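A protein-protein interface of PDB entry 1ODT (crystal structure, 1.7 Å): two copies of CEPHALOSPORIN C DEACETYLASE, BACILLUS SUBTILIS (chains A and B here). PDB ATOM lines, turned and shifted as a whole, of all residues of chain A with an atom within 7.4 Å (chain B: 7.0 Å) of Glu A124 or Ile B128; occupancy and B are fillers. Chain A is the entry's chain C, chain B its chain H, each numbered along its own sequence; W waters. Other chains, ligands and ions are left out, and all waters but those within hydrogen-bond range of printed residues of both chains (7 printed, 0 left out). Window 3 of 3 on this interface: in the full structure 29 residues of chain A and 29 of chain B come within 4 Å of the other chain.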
ATOM      1  N   TYR A  61     -16.895   1.250   9.370  1.00  0.00           N
ATOM      2  CA  TYR A  61     -17.345   1.465  10.748  1.00  0.00           C
ATOM      3  C   TYR A  61     -17.423   2.944  11.080  1.00  0.00           C
ATOM      4  O   TYR A  61     -16.939   3.787  10.317  1.00  0.00           O
ATOM      5  CB  TYR A  61     -16.453   0.779  11.763  1.00  0.00           C
ATOM      6  CG  TYR A  61     -15.012   1.207  11.728  1.00  0.00           C
ATOM      7  CD1 TYR A  61     -14.552   2.294  12.460  1.00  0.00           C
ATOM      8  CD2 TYR A  61     -14.096   0.494  10.970  1.00  0.00           C
ATOM      9  CE1 TYR A  61     -13.244   2.657  12.415  1.00  0.00           C
ATOM     10  CE2 TYR A  61     -12.788   0.834  10.943  1.00  0.00           C
ATOM     11  CZ  TYR A  61     -12.344   1.892  11.685  1.00  0.00           C
ATOM     12  OH  TYR A  61     -10.998   2.215  11.583  1.00  0.00           O
ATOM     13  N   LYS A  62     -18.091   3.271  12.182  1.00  0.00           N
ATOM     14  CA  LYS A  62     -18.211   4.649  12.607  1.00  0.00           C
ATOM     15  C   LYS A  62     -17.200   4.897  13.700  1.00  0.00           C
ATOM     16  O   LYS A  62     -16.945   4.052  14.548  1.00  0.00           O
ATOM     17  CB  LYS A  62     -19.633   4.977  13.095  1.00  0.00           C
ATOM     18  CG  LYS A  62     -20.707   4.794  12.013  1.00  0.00           C
ATOM     19  CD  LYS A  62     -20.301   5.569  10.725  1.00  0.00           C
ATOM     20  CE  LYS A  62     -21.362   6.542  10.179  1.00  0.00           C
ATOM     21  NZ  LYS A  62     -21.991   7.484  11.159  1.00  0.00           N
ATOM     22  N   PHE A  64     -14.740   8.378  15.799  1.00  0.00           N
ATOM     23  CA  PHE A  64     -14.771   9.715  16.344  1.00  0.00           C
ATOM     24  C   PHE A  64     -15.407  10.733  15.400  1.00  0.00           C
ATOM     25  O   PHE A  64     -15.104  10.790  14.223  1.00  0.00           O
ATOM     26  CB  PHE A  64     -13.330  10.121  16.664  1.00  0.00           C
ATOM     27  CG  PHE A  64     -13.179  11.544  17.106  1.00  0.00           C
ATOM     28  CD1 PHE A  64     -13.344  11.904  18.430  1.00  0.00           C
ATOM     29  CD2 PHE A  64     -12.774  12.501  16.183  1.00  0.00           C
ATOM     30  CE1 PHE A  64     -13.171  13.228  18.824  1.00  0.00           C
ATOM     31  CE2 PHE A  64     -12.574  13.827  16.576  1.00  0.00           C
ATOM     32  CZ  PHE A  64     -12.752  14.177  17.892  1.00  0.00           C
ATOM     33  N   GLY A  65     -16.281  11.570  15.958  1.00  0.00           N
ATOM     34  CA  GLY A  65     -16.936  12.577  15.175  1.00  0.00           C
ATOM     35  C   GLY A  65     -17.951  12.013  14.198  1.00  0.00           C
ATOM     36  O   GLY A  65     -18.328  12.667  13.226  1.00  0.00           O
ATOM     37  N   ASN A  66     -18.384  10.790  14.474  1.00  0.00           N
ATOM     38  CA  ASN A  66     -19.307  10.036  13.638  1.00  0.00           C
ATOM     39  C   ASN A  66     -18.839   9.855  12.219  1.00  0.00           C
ATOM     40  O   ASN A  66     -19.650   9.723  11.297  1.00  0.00           O
ATOM     41  CB  ASN A  66     -20.694  10.679  13.658  1.00  0.00           C
ATOM     42  CG  ASN A  66     -21.312  10.670  15.062  1.00  0.00           C
ATOM     43  OD1 ASN A  66     -21.424   9.616  15.701  1.00  0.00           O
ATOM     44  ND2 ASN A  66     -21.741  11.842  15.527  1.00  0.00           N
ATOM     45  N   ALA A  67     -17.539   9.804  12.043  1.00  0.00           N
ATOM     46  CA  ALA A  67     -16.921   9.656  10.729  1.00  0.00           C
ATOM     47  C   ALA A  67     -17.064   8.202  10.238  1.00  0.00           C
ATOM     48  O   ALA A  67     -16.906   7.252  11.033  1.00  0.00           O
ATOM     49  CB  ALA A  67     -15.449  10.057  10.791  1.00  0.00           C
ATOM     50  N   ARG A  68     -17.369   8.052   8.950  1.00  0.00           N
ATOM     51  CA  ARG A  68     -17.429   6.769   8.270  1.00  0.00           C
ATOM     52  C   ARG A  68     -16.022   6.393   7.814  1.00  0.00           C
ATOM     53  O   ARG A  68     -15.441   7.019   6.943  1.00  0.00           O
ATOM     54  CB  ARG A  68     -18.349   6.870   7.065  1.00  0.00           C
ATOM     55  CG  ARG A  68     -18.483   5.627   6.188  1.00  0.00           C
ATOM     56  CD  ARG A  68     -19.206   5.882   4.863  1.00  0.00           C
ATOM     57  NE  ARG A  68     -18.494   6.904   4.119  1.00  0.00           N
ATOM     58  CZ  ARG A  68     -17.351   6.716   3.458  1.00  0.00           C
ATOM     59  NH1 ARG A  68     -16.808   5.505   3.305  1.00  0.00           N
ATOM     60  NH2 ARG A  68     -16.800   7.748   2.860  1.00  0.00           N
ATOM     61  N   ILE A  69     -15.479   5.354   8.405  1.00  0.00           N
ATOM     62  CA  ILE A  69     -14.142   4.915   8.070  1.00  0.00           C
ATOM     63  C   ILE A  69     -14.222   3.572   7.391  1.00  0.00           C
ATOM     64  O   ILE A  69     -15.021   2.750   7.764  1.00  0.00           O
ATOM     65  CB  ILE A  69     -13.174   4.931   9.325  1.00  0.00           C
ATOM     66  CG1 ILE A  69     -12.182   3.808   9.276  1.00  0.00           C
ATOM     67  CG2 ILE A  69     -13.876   5.281  10.595  1.00  0.00           C
ATOM     68  CD1 ILE A  69     -11.105   4.092   8.305  1.00  0.00           C
ATOM     69  N   THR A  70     -13.417   3.379   6.347  1.00  0.00           N
ATOM     70  CA  THR A  70     -13.525   2.179   5.549  1.00  0.00           C
ATOM     71  C   THR A  70     -12.170   1.641   5.113  1.00  0.00           C
ATOM     72  O   THR A  70     -11.132   2.241   5.362  1.00  0.00           O
ATOM     73  CB  THR A  70     -14.492   2.458   4.354  1.00  0.00           C
ATOM     74  OG1 THR A  70     -14.903   1.234   3.709  1.00  0.00           O
ATOM     75  CG2 THR A  70     -13.815   3.306   3.285  1.00  0.00           C
ATOM     76  N   LEU A 116      -8.211   2.922   5.805  1.00  0.00           N
ATOM     77  CA  LEU A 116      -7.968   4.062   4.955  1.00  0.00           C
ATOM     78  C   LEU A 116      -8.172   5.351   5.726  1.00  0.00           C
ATOM     79  O   LEU A 116      -9.143   5.502   6.504  1.00  0.00           O
ATOM     80  CB  LEU A 116      -8.860   3.946   3.721  1.00  0.00           C
ATOM     81  CG  LEU A 116      -8.704   2.599   3.002  1.00  0.00           C
ATOM     82  CD1 LEU A 116      -9.566   2.534   1.743  1.00  0.00           C
ATOM     83  CD2 LEU A 116      -7.246   2.350   2.637  1.00  0.00           C
ATOM     84  N   VAL A 117      -7.236   6.296   5.573  1.00  0.00           N
ATOM     85  CA  VAL A 117      -7.194   7.460   6.455  1.00  0.00           C
ATOM     86  C   VAL A 117      -8.191   8.506   6.036  1.00  0.00           C
ATOM     87  O   VAL A 117      -8.276   8.879   4.833  1.00  0.00           O
ATOM     88  CB  VAL A 117      -5.776   8.063   6.561  1.00  0.00           C
ATOM     89  CG1 VAL A 117      -5.772   9.310   7.475  1.00  0.00           C
ATOM     90  CG2 VAL A 117      -4.792   7.004   7.068  1.00  0.00           C
ATOM     91  N   ARG A 118      -9.002   8.904   7.017  1.00  0.00           N
ATOM     92  CA  ARG A 118     -10.043   9.908   6.842  1.00  0.00           C
ATOM     93  C   ARG A 118      -9.551  11.103   6.030  1.00  0.00           C
ATOM     94  O   ARG A 118      -8.553  11.699   6.328  1.00  0.00           O
ATOM     95  CB  ARG A 118     -10.610  10.355   8.173  1.00  0.00           C
ATOM     96  CG  ARG A 118      -9.594  10.848   9.177  1.00  0.00           C
ATOM     97  CD  ARG A 118     -10.192  11.678  10.246  1.00  0.00           C
ATOM     98  NE  ARG A 118     -10.976  10.868  11.154  1.00  0.00           N
ATOM     99  CZ  ARG A 118     -11.984  11.314  11.899  1.00  0.00           C
ATOM    100  NH1 ARG A 118     -12.406  12.566  11.809  1.00  0.00           N
ATOM    101  NH2 ARG A 118     -12.572  10.486  12.752  1.00  0.00           N
ATOM    102  N   GLY A 119     -10.261  11.418   4.954  1.00  0.00           N
ATOM    103  CA  GLY A 119      -9.916  12.572   4.162  1.00  0.00           C
ATOM    104  C   GLY A 119      -8.897  12.312   3.068  1.00  0.00           C
ATOM    105  O   GLY A 119      -8.851  13.093   2.139  1.00  0.00           O
ATOM    106  N   GLN A 120      -8.097  11.245   3.182  1.00  0.00           N
ATOM    107  CA  GLN A 120      -7.043  10.921   2.192  1.00  0.00           C
ATOM    108  C   GLN A 120      -7.514   9.919   1.124  1.00  0.00           C
ATOM    109  O   GLN A 120      -7.233  10.054  -0.052  1.00  0.00           O
ATOM    110  CB  GLN A 120      -5.787  10.388   2.876  1.00  0.00           C
ATOM    111  CG  GLN A 120      -5.167  11.363   3.850  1.00  0.00           C
ATOM    112  CD  GLN A 120      -3.896  10.923   4.539  1.00  0.00           C
ATOM    113  OE1 GLN A 120      -3.577  11.461   5.631  1.00  0.00           O
ATOM    114  NE2 GLN A 120      -3.161   9.999   3.949  1.00  0.00           N
ATOM    115  N   GLN A 121      -8.232   8.893   1.549  1.00  0.00           N
ATOM    116  CA  GLN A 121      -8.636   7.834   0.681  1.00  0.00           C
ATOM    117  C   GLN A 121      -9.903   7.169   1.240  1.00  0.00           C
ATOM    118  O   GLN A 121      -9.885   6.610   2.313  1.00  0.00           O
ATOM    119  CB  GLN A 121      -7.481   6.847   0.585  1.00  0.00           C
ATOM    120  CG  GLN A 121      -7.715   5.575  -0.138  1.00  0.00           C
ATOM    121  CD  GLN A 121      -8.176   5.768  -1.532  1.00  0.00           C
ATOM    122  OE1 GLN A 121      -9.235   5.293  -1.893  1.00  0.00           O
ATOM    123  NE2 GLN A 121      -7.423   6.519  -2.315  1.00  0.00           N
ATOM    124  N   SER A 122     -11.008   7.304   0.517  1.00  0.00           N
ATOM    125  CA  SER A 122     -12.267   6.650   0.816  1.00  0.00           C
ATOM    126  C   SER A 122     -12.978   7.059   2.097  1.00  0.00           C
ATOM    127  O   SER A 122     -14.145   7.457   2.036  1.00  0.00           O
ATOM    128  CB  SER A 122     -12.117   5.126   0.735  1.00  0.00           C
ATOM    129  OG  SER A 122     -11.843   4.765  -0.601  1.00  0.00           O
ATOM    130  N   SER A 123     -12.280   7.039   3.222  1.00  0.00           N
ATOM    131  CA  SER A 123     -12.856   7.352   4.498  1.00  0.00           C
ATOM    132  C   SER A 123     -13.164   8.842   4.592  1.00  0.00           C
ATOM    133  O   SER A 123     -12.440   9.694   4.045  1.00  0.00           O
ATOM    134  CB  SER A 123     -11.867   6.954   5.604  1.00  0.00           C
ATOM    135  OG  SER A 123     -11.666   5.549   5.512  1.00  0.00           O
ATOM    136  N   GLU A 124     -14.197   9.132   5.349  1.00  0.00           N
ATOM    137  CA  GLU A 124     -14.695  10.478   5.581  1.00  0.00           C
ATOM    138  C   GLU A 124     -14.000  11.155   6.763  1.00  0.00           C
ATOM    139  O   GLU A 124     -13.864  10.563   7.813  1.00  0.00           O
ATOM    140  CB  GLU A 124     -16.174  10.352   5.928  1.00  0.00           C
ATOM    141  CG  GLU A 124     -16.937  11.607   6.300  1.00  0.00           C
ATOM    142  CD  GLU A 124     -18.367  11.249   6.709  1.00  0.00           C
ATOM    143  OE1 GLU A 124     -18.554  10.360   7.574  1.00  0.00           O
ATOM    144  OE2 GLU A 124     -19.294  11.820   6.136  1.00  0.00           O
ATOM    145  N   ASP A 125     -13.628  12.426   6.595  1.00  0.00           N
ATOM    146  CA  ASP A 125     -13.155  13.264   7.723  1.00  0.00           C
ATOM    147  C   ASP A 125     -14.233  14.302   8.035  1.00  0.00           C
ATOM    148  O   ASP A 125     -14.491  15.235   7.237  1.00  0.00           O
ATOM    149  CB  ASP A 125     -11.846  13.938   7.351  1.00  0.00           C
ATOM    150  CG  ASP A 125     -11.295  14.782   8.439  1.00  0.00           C
ATOM    151  OD1 ASP A 125     -11.784  14.711   9.616  1.00  0.00           O
ATOM    152  OD2 ASP A 125     -10.373  15.572   8.221  1.00  0.00           O
ATOM    153  N   THR A 126     -14.956  14.065   9.122  1.00  0.00           N
ATOM    154  CA  THR A 126     -15.998  14.960   9.574  1.00  0.00           C
ATOM    155  C   THR A 126     -15.469  16.126  10.377  1.00  0.00           C
ATOM    156  O   THR A 126     -16.226  16.999  10.722  1.00  0.00           O
ATOM    157  CB  THR A 126     -17.044  14.182  10.442  1.00  0.00           C
ATOM    158  OG1 THR A 126     -16.362  13.548  11.561  1.00  0.00           O
ATOM    159  CG2 THR A 126     -17.731  13.122   9.638  1.00  0.00           C
ATOM    160  N   SER A 127     -14.173  16.154  10.701  1.00  0.00           N
ATOM    161  CA  SER A 127     -13.650  17.273  11.472  1.00  0.00           C
ATOM    162  C   SER A 127     -13.518  18.482  10.523  1.00  0.00           C
ATOM    163  O   SER A 127     -13.133  18.348   9.362  1.00  0.00           O
ATOM    164  CB  SER A 127     -12.331  16.916  12.137  1.00  0.00           C
ATOM    165  OG  SER A 127     -11.277  16.746  11.175  1.00  0.00           O
ATOM    166  N   ILE A 128     -13.860  19.673  11.003  1.00  0.00           N
ATOM    167  CA  ILE A 128     -13.868  20.836  10.111  1.00  0.00           C
ATOM    168  C   ILE A 128     -12.462  21.434   9.931  1.00  0.00           C
ATOM    169  O   ILE A 128     -11.507  20.927  10.518  1.00  0.00           O
ATOM    170  CB  ILE A 128     -14.896  21.875  10.604  1.00  0.00           C
ATOM    171  CG1 ILE A 128     -14.545  22.389  11.986  1.00  0.00           C
ATOM    172  CG2 ILE A 128     -16.301  21.244  10.614  1.00  0.00           C
ATOM    173  CD1 ILE A 128     -15.005  23.813  12.232  1.00  0.00           C
ATOM    174  N   SER A 129     -12.306  22.416   9.033  1.00  0.00           N
ATOM    175  CA  SER A 129     -11.083  23.238   9.045  1.00  0.00           C
ATOM    176  C   SER A 129     -11.384  24.526   9.865  1.00  0.00           C
ATOM    177  O   SER A 129     -11.917  25.461   9.312  1.00  0.00           O
ATOM    178  CB  SER A 129     -10.643  23.538   7.601  1.00  0.00           C
ATOM    179  OG  SER A 129     -10.524  22.334   6.833  1.00  0.00           O
ATOM    180  N   LYS A 140      -4.036  21.121   9.441  1.00  0.00           N
ATOM    181  CA  LYS A 140      -5.483  21.193   9.620  1.00  0.00           C
ATOM    182  C   LYS A 140      -5.825  21.084  11.102  1.00  0.00           C
ATOM    183  O   LYS A 140      -5.528  20.081  11.722  1.00  0.00           O
ATOM    184  CB  LYS A 140      -6.141  20.081   8.831  1.00  0.00           C
ATOM    185  CG  LYS A 140      -7.666  20.053   8.909  1.00  0.00           C
ATOM    186  CD  LYS A 140      -8.326  19.126   7.860  1.00  0.00           C
ATOM    187  CE  LYS A 140      -9.833  19.117   8.023  1.00  0.00           C
ATOM    188  NZ  LYS A 140     -10.205  18.367   9.240  1.00  0.00           N
ATOM    189  N   ASP A 156      -9.484   6.702  14.998  1.00  0.00           N
ATOM    190  CA  ASP A 156      -9.867   5.727  13.977  1.00  0.00           C
ATOM    191  C   ASP A 156      -9.003   4.478  13.984  1.00  0.00           C
ATOM    192  O   ASP A 156      -9.509   3.375  13.834  1.00  0.00           O
ATOM    193  CB  ASP A 156      -9.774   6.280  12.540  1.00  0.00           C
ATOM    194  CG  ASP A 156     -10.580   7.533  12.302  1.00  0.00           C
ATOM    195  OD1 ASP A 156     -11.562   7.833  13.053  1.00  0.00           O
ATOM    196  OD2 ASP A 156     -10.264   8.250  11.306  1.00  0.00           O
ATOM    197  N   ASP B 125     -13.567  26.440   6.996  1.00  0.00           N
ATOM    198  CA  ASP B 125     -14.341  25.577   6.097  1.00  0.00           C
ATOM    199  C   ASP B 125     -15.094  24.529   6.926  1.00  0.00           C
ATOM    200  O   ASP B 125     -14.513  23.547   7.383  1.00  0.00           O
ATOM    201  CB  ASP B 125     -13.406  24.879   5.110  1.00  0.00           C
ATOM    202  CG  ASP B 125     -14.124  24.060   4.091  1.00  0.00           C
ATOM    203  OD1 ASP B 125     -15.365  24.068   4.026  1.00  0.00           O
ATOM    204  OD2 ASP B 125     -13.495  23.309   3.337  1.00  0.00           O
ATOM    205  N   THR B 126     -16.417  24.712   7.072  1.00  0.00           N
ATOM    206  CA  THR B 126     -17.261  23.761   7.774  1.00  0.00           C
ATOM    207  C   THR B 126     -17.738  22.589   6.922  1.00  0.00           C
ATOM    208  O   THR B 126     -18.380  21.688   7.439  1.00  0.00           O
ATOM    209  CB  THR B 126     -18.536  24.452   8.356  1.00  0.00           C
ATOM    210  OG1 THR B 126     -19.246  25.115   7.300  1.00  0.00           O
ATOM    211  CG2 THR B 126     -18.181  25.499   9.439  1.00  0.00           C
ATOM    212  N   SER B 127     -17.462  22.619   5.618  1.00  0.00           N
ATOM    213  CA  SER B 127     -17.869  21.530   4.758  1.00  0.00           C
ATOM    214  C   SER B 127     -16.961  20.317   5.031  1.00  0.00           C
ATOM    215  O   SER B 127     -15.742  20.485   5.212  1.00  0.00           O
ATOM    216  CB  SER B 127     -17.870  21.971   3.316  1.00  0.00           C
ATOM    217  OG  SER B 127     -16.574  22.060   2.789  1.00  0.00           O
ATOM    218  N   ILE B 128     -17.547  19.120   5.095  1.00  0.00           N
ATOM    219  CA  ILE B 128     -16.736  17.938   5.492  1.00  0.00           C
ATOM    220  C   ILE B 128     -15.920  17.393   4.310  1.00  0.00           C
ATOM    221  O   ILE B 128     -15.959  17.969   3.228  1.00  0.00           O
ATOM    222  CB  ILE B 128     -17.601  16.834   6.189  1.00  0.00           C
ATOM    223  CG1 ILE B 128     -18.678  16.267   5.251  1.00  0.00           C
ATOM    224  CG2 ILE B 128     -18.159  17.396   7.494  1.00  0.00           C
ATOM    225  CD1 ILE B 128     -19.492  15.107   5.813  1.00  0.00           C
ATOM    226  N   SER B 129     -15.082  16.375   4.546  1.00  0.00           N
ATOM    227  CA  SER B 129     -14.515  15.558   3.450  1.00  0.00           C
ATOM    228  C   SER B 129     -15.345  14.241   3.375  1.00  0.00           C
ATOM    229  O   SER B 129     -15.078  13.338   4.143  1.00  0.00           O
ATOM    230  CB  SER B 129     -13.051  15.210   3.742  1.00  0.00           C
ATOM    231  OG  SER B 129     -12.259  16.360   3.976  1.00  0.00           O
ATOM    232  N   PRO B 130     -16.336  14.173   2.497  1.00  0.00           N
ATOM    233  CA  PRO B 130     -17.302  13.064   2.459  1.00  0.00           C
ATOM    234  C   PRO B 130     -16.693  11.753   1.957  1.00  0.00           C
ATOM    235  O   PRO B 130     -17.142  10.702   2.381  1.00  0.00           O
ATOM    236  CB  PRO B 130     -18.391  13.578   1.529  1.00  0.00           C
ATOM    237  CG  PRO B 130     -17.733  14.501   0.646  1.00  0.00           C
ATOM    238  CD  PRO B 130     -16.639  15.202   1.496  1.00  0.00           C
ATOM    239  N   HIS B 131     -15.638  11.810   1.150  1.00  0.00           N
ATOM    240  CA  HIS B 131     -15.102  10.599   0.509  1.00  0.00           C
ATOM    241  C   HIS B 131     -13.584  10.412   0.406  1.00  0.00           C
ATOM    242  O   HIS B 131     -13.159   9.392  -0.171  1.00  0.00           O
ATOM    243  CB  HIS B 131     -15.619  10.454  -0.934  1.00  0.00           C
ATOM    244  CG  HIS B 131     -15.477  11.680  -1.753  1.00  0.00           C
ATOM    245  ND1 HIS B 131     -14.267  12.140  -2.220  1.00  0.00           N
ATOM    246  CD2 HIS B 131     -16.418  12.528  -2.231  1.00  0.00           C
ATOM    247  CE1 HIS B 131     -14.472  13.232  -2.941  1.00  0.00           C
ATOM    248  NE2 HIS B 131     -15.767  13.492  -2.951  1.00  0.00           N
ATOM    249  N   GLY B 132     -12.782  11.334   0.914  1.00  0.00           N
ATOM    250  CA  GLY B 132     -11.338  11.216   0.780  1.00  0.00           C
ATOM    251  C   GLY B 132     -10.930  11.801  -0.560  1.00  0.00           C
ATOM    252  O   GLY B 132     -11.603  11.630  -1.577  1.00  0.00           O
ATOM    253  N   HIS B 133      -9.811  12.503  -0.576  1.00  0.00           N
ATOM    254  CA  HIS B 133      -9.417  13.254  -1.774  1.00  0.00           C
ATOM    255  C   HIS B 133      -7.894  13.299  -1.885  1.00  0.00           C
ATOM    256  O   HIS B 133      -7.180  13.028  -0.893  1.00  0.00           O
ATOM    257  CB  HIS B 133     -10.048  14.676  -1.770  1.00  0.00           C
ATOM    258  CG  HIS B 133      -9.760  15.486  -0.531  1.00  0.00           C
ATOM    259  ND1 HIS B 133      -8.597  16.199  -0.363  1.00  0.00           N
ATOM    260  CD2 HIS B 133     -10.486  15.688   0.602  1.00  0.00           C
ATOM    261  CE1 HIS B 133      -8.624  16.819   0.810  1.00  0.00           C
ATOM    262  NE2 HIS B 133      -9.765  16.539   1.402  1.00  0.00           N
ATOM    263  N   LYS B 140     -11.612  17.917  -2.974  1.00  0.00           N
ATOM    264  CA  LYS B 140     -12.448  17.808  -1.786  1.00  0.00           C
ATOM    265  C   LYS B 140     -13.946  17.890  -2.116  1.00  0.00           C
ATOM    266  O   LYS B 140     -14.431  18.919  -2.589  1.00  0.00           O
ATOM    267  CB  LYS B 140     -12.034  18.868  -0.746  1.00  0.00           C
ATOM    268  CG  LYS B 140     -12.844  18.855   0.526  1.00  0.00           C
ATOM    269  CD  LYS B 140     -12.186  19.731   1.617  1.00  0.00           C
ATOM    270  CE  LYS B 140     -12.921  19.636   2.923  1.00  0.00           C
ATOM    271  NZ  LYS B 140     -14.002  20.567   2.963  1.00  0.00           N
ATOM    272  N   GLY B 141     -14.677  16.808  -1.850  1.00  0.00           N
ATOM    273  CA  GLY B 141     -16.096  16.743  -2.146  1.00  0.00           C
ATOM    274  C   GLY B 141     -16.446  16.633  -3.614  1.00  0.00           C
ATOM    275  O   GLY B 141     -17.604  16.834  -3.985  1.00  0.00           O
ATOM    276  N   THR B 147     -21.449  18.862  -2.203  1.00  0.00           N
ATOM    277  CA  THR B 147     -20.376  18.753  -1.217  1.00  0.00           C
ATOM    278  C   THR B 147     -19.054  19.361  -1.693  1.00  0.00           C
ATOM    279  O   THR B 147     -18.087  19.421  -0.923  1.00  0.00           O
ATOM    280  CB  THR B 147     -20.107  17.261  -0.863  1.00  0.00           C
ATOM    281  OG1 THR B 147     -19.813  16.500  -2.038  1.00  0.00           O
ATOM    282  CG2 THR B 147     -21.323  16.571  -0.295  1.00  0.00           C
ATOM    283  N   TYR B 149     -15.877  21.502  -2.631  1.00  0.00           N
ATOM    284  CA  TYR B 149     -15.204  22.594  -1.962  1.00  0.00           C
ATOM    285  C   TYR B 149     -15.584  23.978  -2.448  1.00  0.00           C
ATOM    286  O   TYR B 149     -15.889  24.845  -1.637  1.00  0.00           O
ATOM    287  CB  TYR B 149     -13.736  22.433  -2.160  1.00  0.00           C
ATOM    288  CG  TYR B 149     -12.906  23.534  -1.555  1.00  0.00           C
ATOM    289  CD1 TYR B 149     -12.872  23.723  -0.188  1.00  0.00           C
ATOM    290  CD2 TYR B 149     -12.128  24.354  -2.359  1.00  0.00           C
ATOM    291  CE1 TYR B 149     -12.089  24.690   0.371  1.00  0.00           C
ATOM    292  CE2 TYR B 149     -11.351  25.355  -1.813  1.00  0.00           C
ATOM    293  CZ  TYR B 149     -11.314  25.493  -0.441  1.00  0.00           C
ATOM    294  OH  TYR B 149     -10.543  26.473   0.112  1.00  0.00           O
HETATM  295  O   HOH W   1     -19.276   9.698   3.926  1.00  0.00           O
HETATM  296  O   HOH W   2     -12.967  18.097   6.663  1.00  0.00           O
HETATM  297  O   HOH W   3     -10.878   8.750  -1.951  1.00  0.00           O
HETATM  298  O   HOH W   4     -10.697  23.173   3.818  1.00  0.00           O
HETATM  299  O   HOH W   5      -4.815  10.775  -1.022  1.00  0.00           O
HETATM  300  O   HOH W   6     -13.114  20.952   6.309  1.00  0.00           O
HETATM  301  O   HOH W   7      -9.623  15.688   5.497  1.00  0.00           O
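Water W5 bridges O of Gln A120 (2.7 Å) and O of His B133 (3.3 Å).
Water W2 lies within hydrogen-bond range of the backbone carbonyl oxygen (O) of Ser A127, the side-chain hydroxyl (OG) of Ser B129 and the backbone carbonyl oxygen (O) of Asp A125.
Water W7 bridges the side-chain carboxylate of Asp A125 and the side-chain hydroxyl of Ser B129.
Water W4 bridges the side-chain carboxylate (OD2) of Asp B125 and the side-chain hydroxyl (OG) of Ser A129.
Water W3 lies within hydrogen-bond range of the backbone NH (N) of Ser A122, the backbone carbonyl oxygen (O) of His B131 and the backbone carbonyl oxygen (O) of Gly B132.
Water W6 lies within hydrogen-bond range of the backbone carbonyl oxygen of Ser B127 (2.9 Å), the side-chain hydroxyl of Ser A129 (3.0 Å), the backbone carbonyl oxygen of Asp B125 (3.1 Å) and the side-chain amino group of Lys B140 (3.5 Å).
O of Pro B130 sits at hydrogen-bond distance from NH2 of Arg A68, at 3.0 Å.
The backbone carbonyl oxygen (O) of Gly A119 is in hydrogen-bond range of the backbone NH (N) of His B133 (2.9 Å).
The backbone carbonyl oxygen (O) of His B131 lies close to the backbone NH (N) of Ser A122 (3.1 Å).
The backbone carbonyl oxygen (O) of Asp A125 is in hydrogen-bond range of the backbone NH (N) of Ser B129.
O of Asp B125 sits at hydrogen-bond distance from N of Ser A129.
The backbone carbonyl oxygen (O) of His B133 sits close to the backbone carbonyl oxygen (O) of Gln A120.
The backbone carbonyl oxygen (O) of Gly A65 sits at hydrogen-bond distance from the side-chain hydroxyl (OG1) of Thr A126 (2.7 Å).
NH2 of Arg A68 is in hydrogen-bond range of O of Ser A122 (2.8 Å).
O of Arg A68 sits at hydrogen-bond distance from N of Glu A124 (2.9 Å).
OG of Ser A123 lies within hydrogen-bond range of O of Leu A116.
OD1 of Asp A125 is in hydrogen-bond range of OG of Ser A127 (2.6 Å).
NZ of Lys A140 is in salt-bridge range of OD2 of Asp A125.
CA of Gly B132 touches O of Gly A119, 3.4 Å away.
Gly B132 touches Gln A121 (CA to N, 3.95 Å).
Ser A122 touches Gly B132 (N to CA, 3.9 Å).
His B131 touches Ser A123 (C to O, 3.9 Å).
Glu A124 touches Ile B128.
Glu A124 touches Ser B129 (CA to O, 3.2 Å).
Ile B128 touches Asp A125 (CB to O, 3.7 Å).
Thr A126 touches Ile B128 (O to CG2, 3.8 Å).
Ile A128 touches Asp B125 (CB to O, 3.6 Å).
Thr B126 touches Ile A128.
Printed residues of chain B that touch a printed residue of chain A: Asp B125, Thr B126, Ile B128, Ser B129, Pro B130, His B131, Gly B132 and His B133.
Among the printed residues, no Asp or Glu carboxylate lies within 4 Å of a Lys or Arg side-chain nitrogen of the other chain.
Asp A125 touches Ile B128, and with the chains exchanged Ile A128 touches Asp B125.
Asp A125 touches Ser B129, and with the chains exchanged Ser A129 touches Asp B125.
Thr A126 touches Ile B128, and with the chains exchanged Ile A128 touches Thr B126.
6 positions are printed for both chains.
Of the printed residues of chain B, Glu A124 touches Ile B128, Ser B129 and Pro B130.
Ile B128 touches three residues of chain A.
Of the printed residues of chain B, Ser A122 touches His B131 and Gly B132.
Printed residues of chain B within 4 Å of Asp A125: Ile B128 (3.7 Å) and Ser B129 (3.0 Å).
The nearest printed residue of chain A that does not touch Asp B125 is Ser A127 (5.7 Å).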
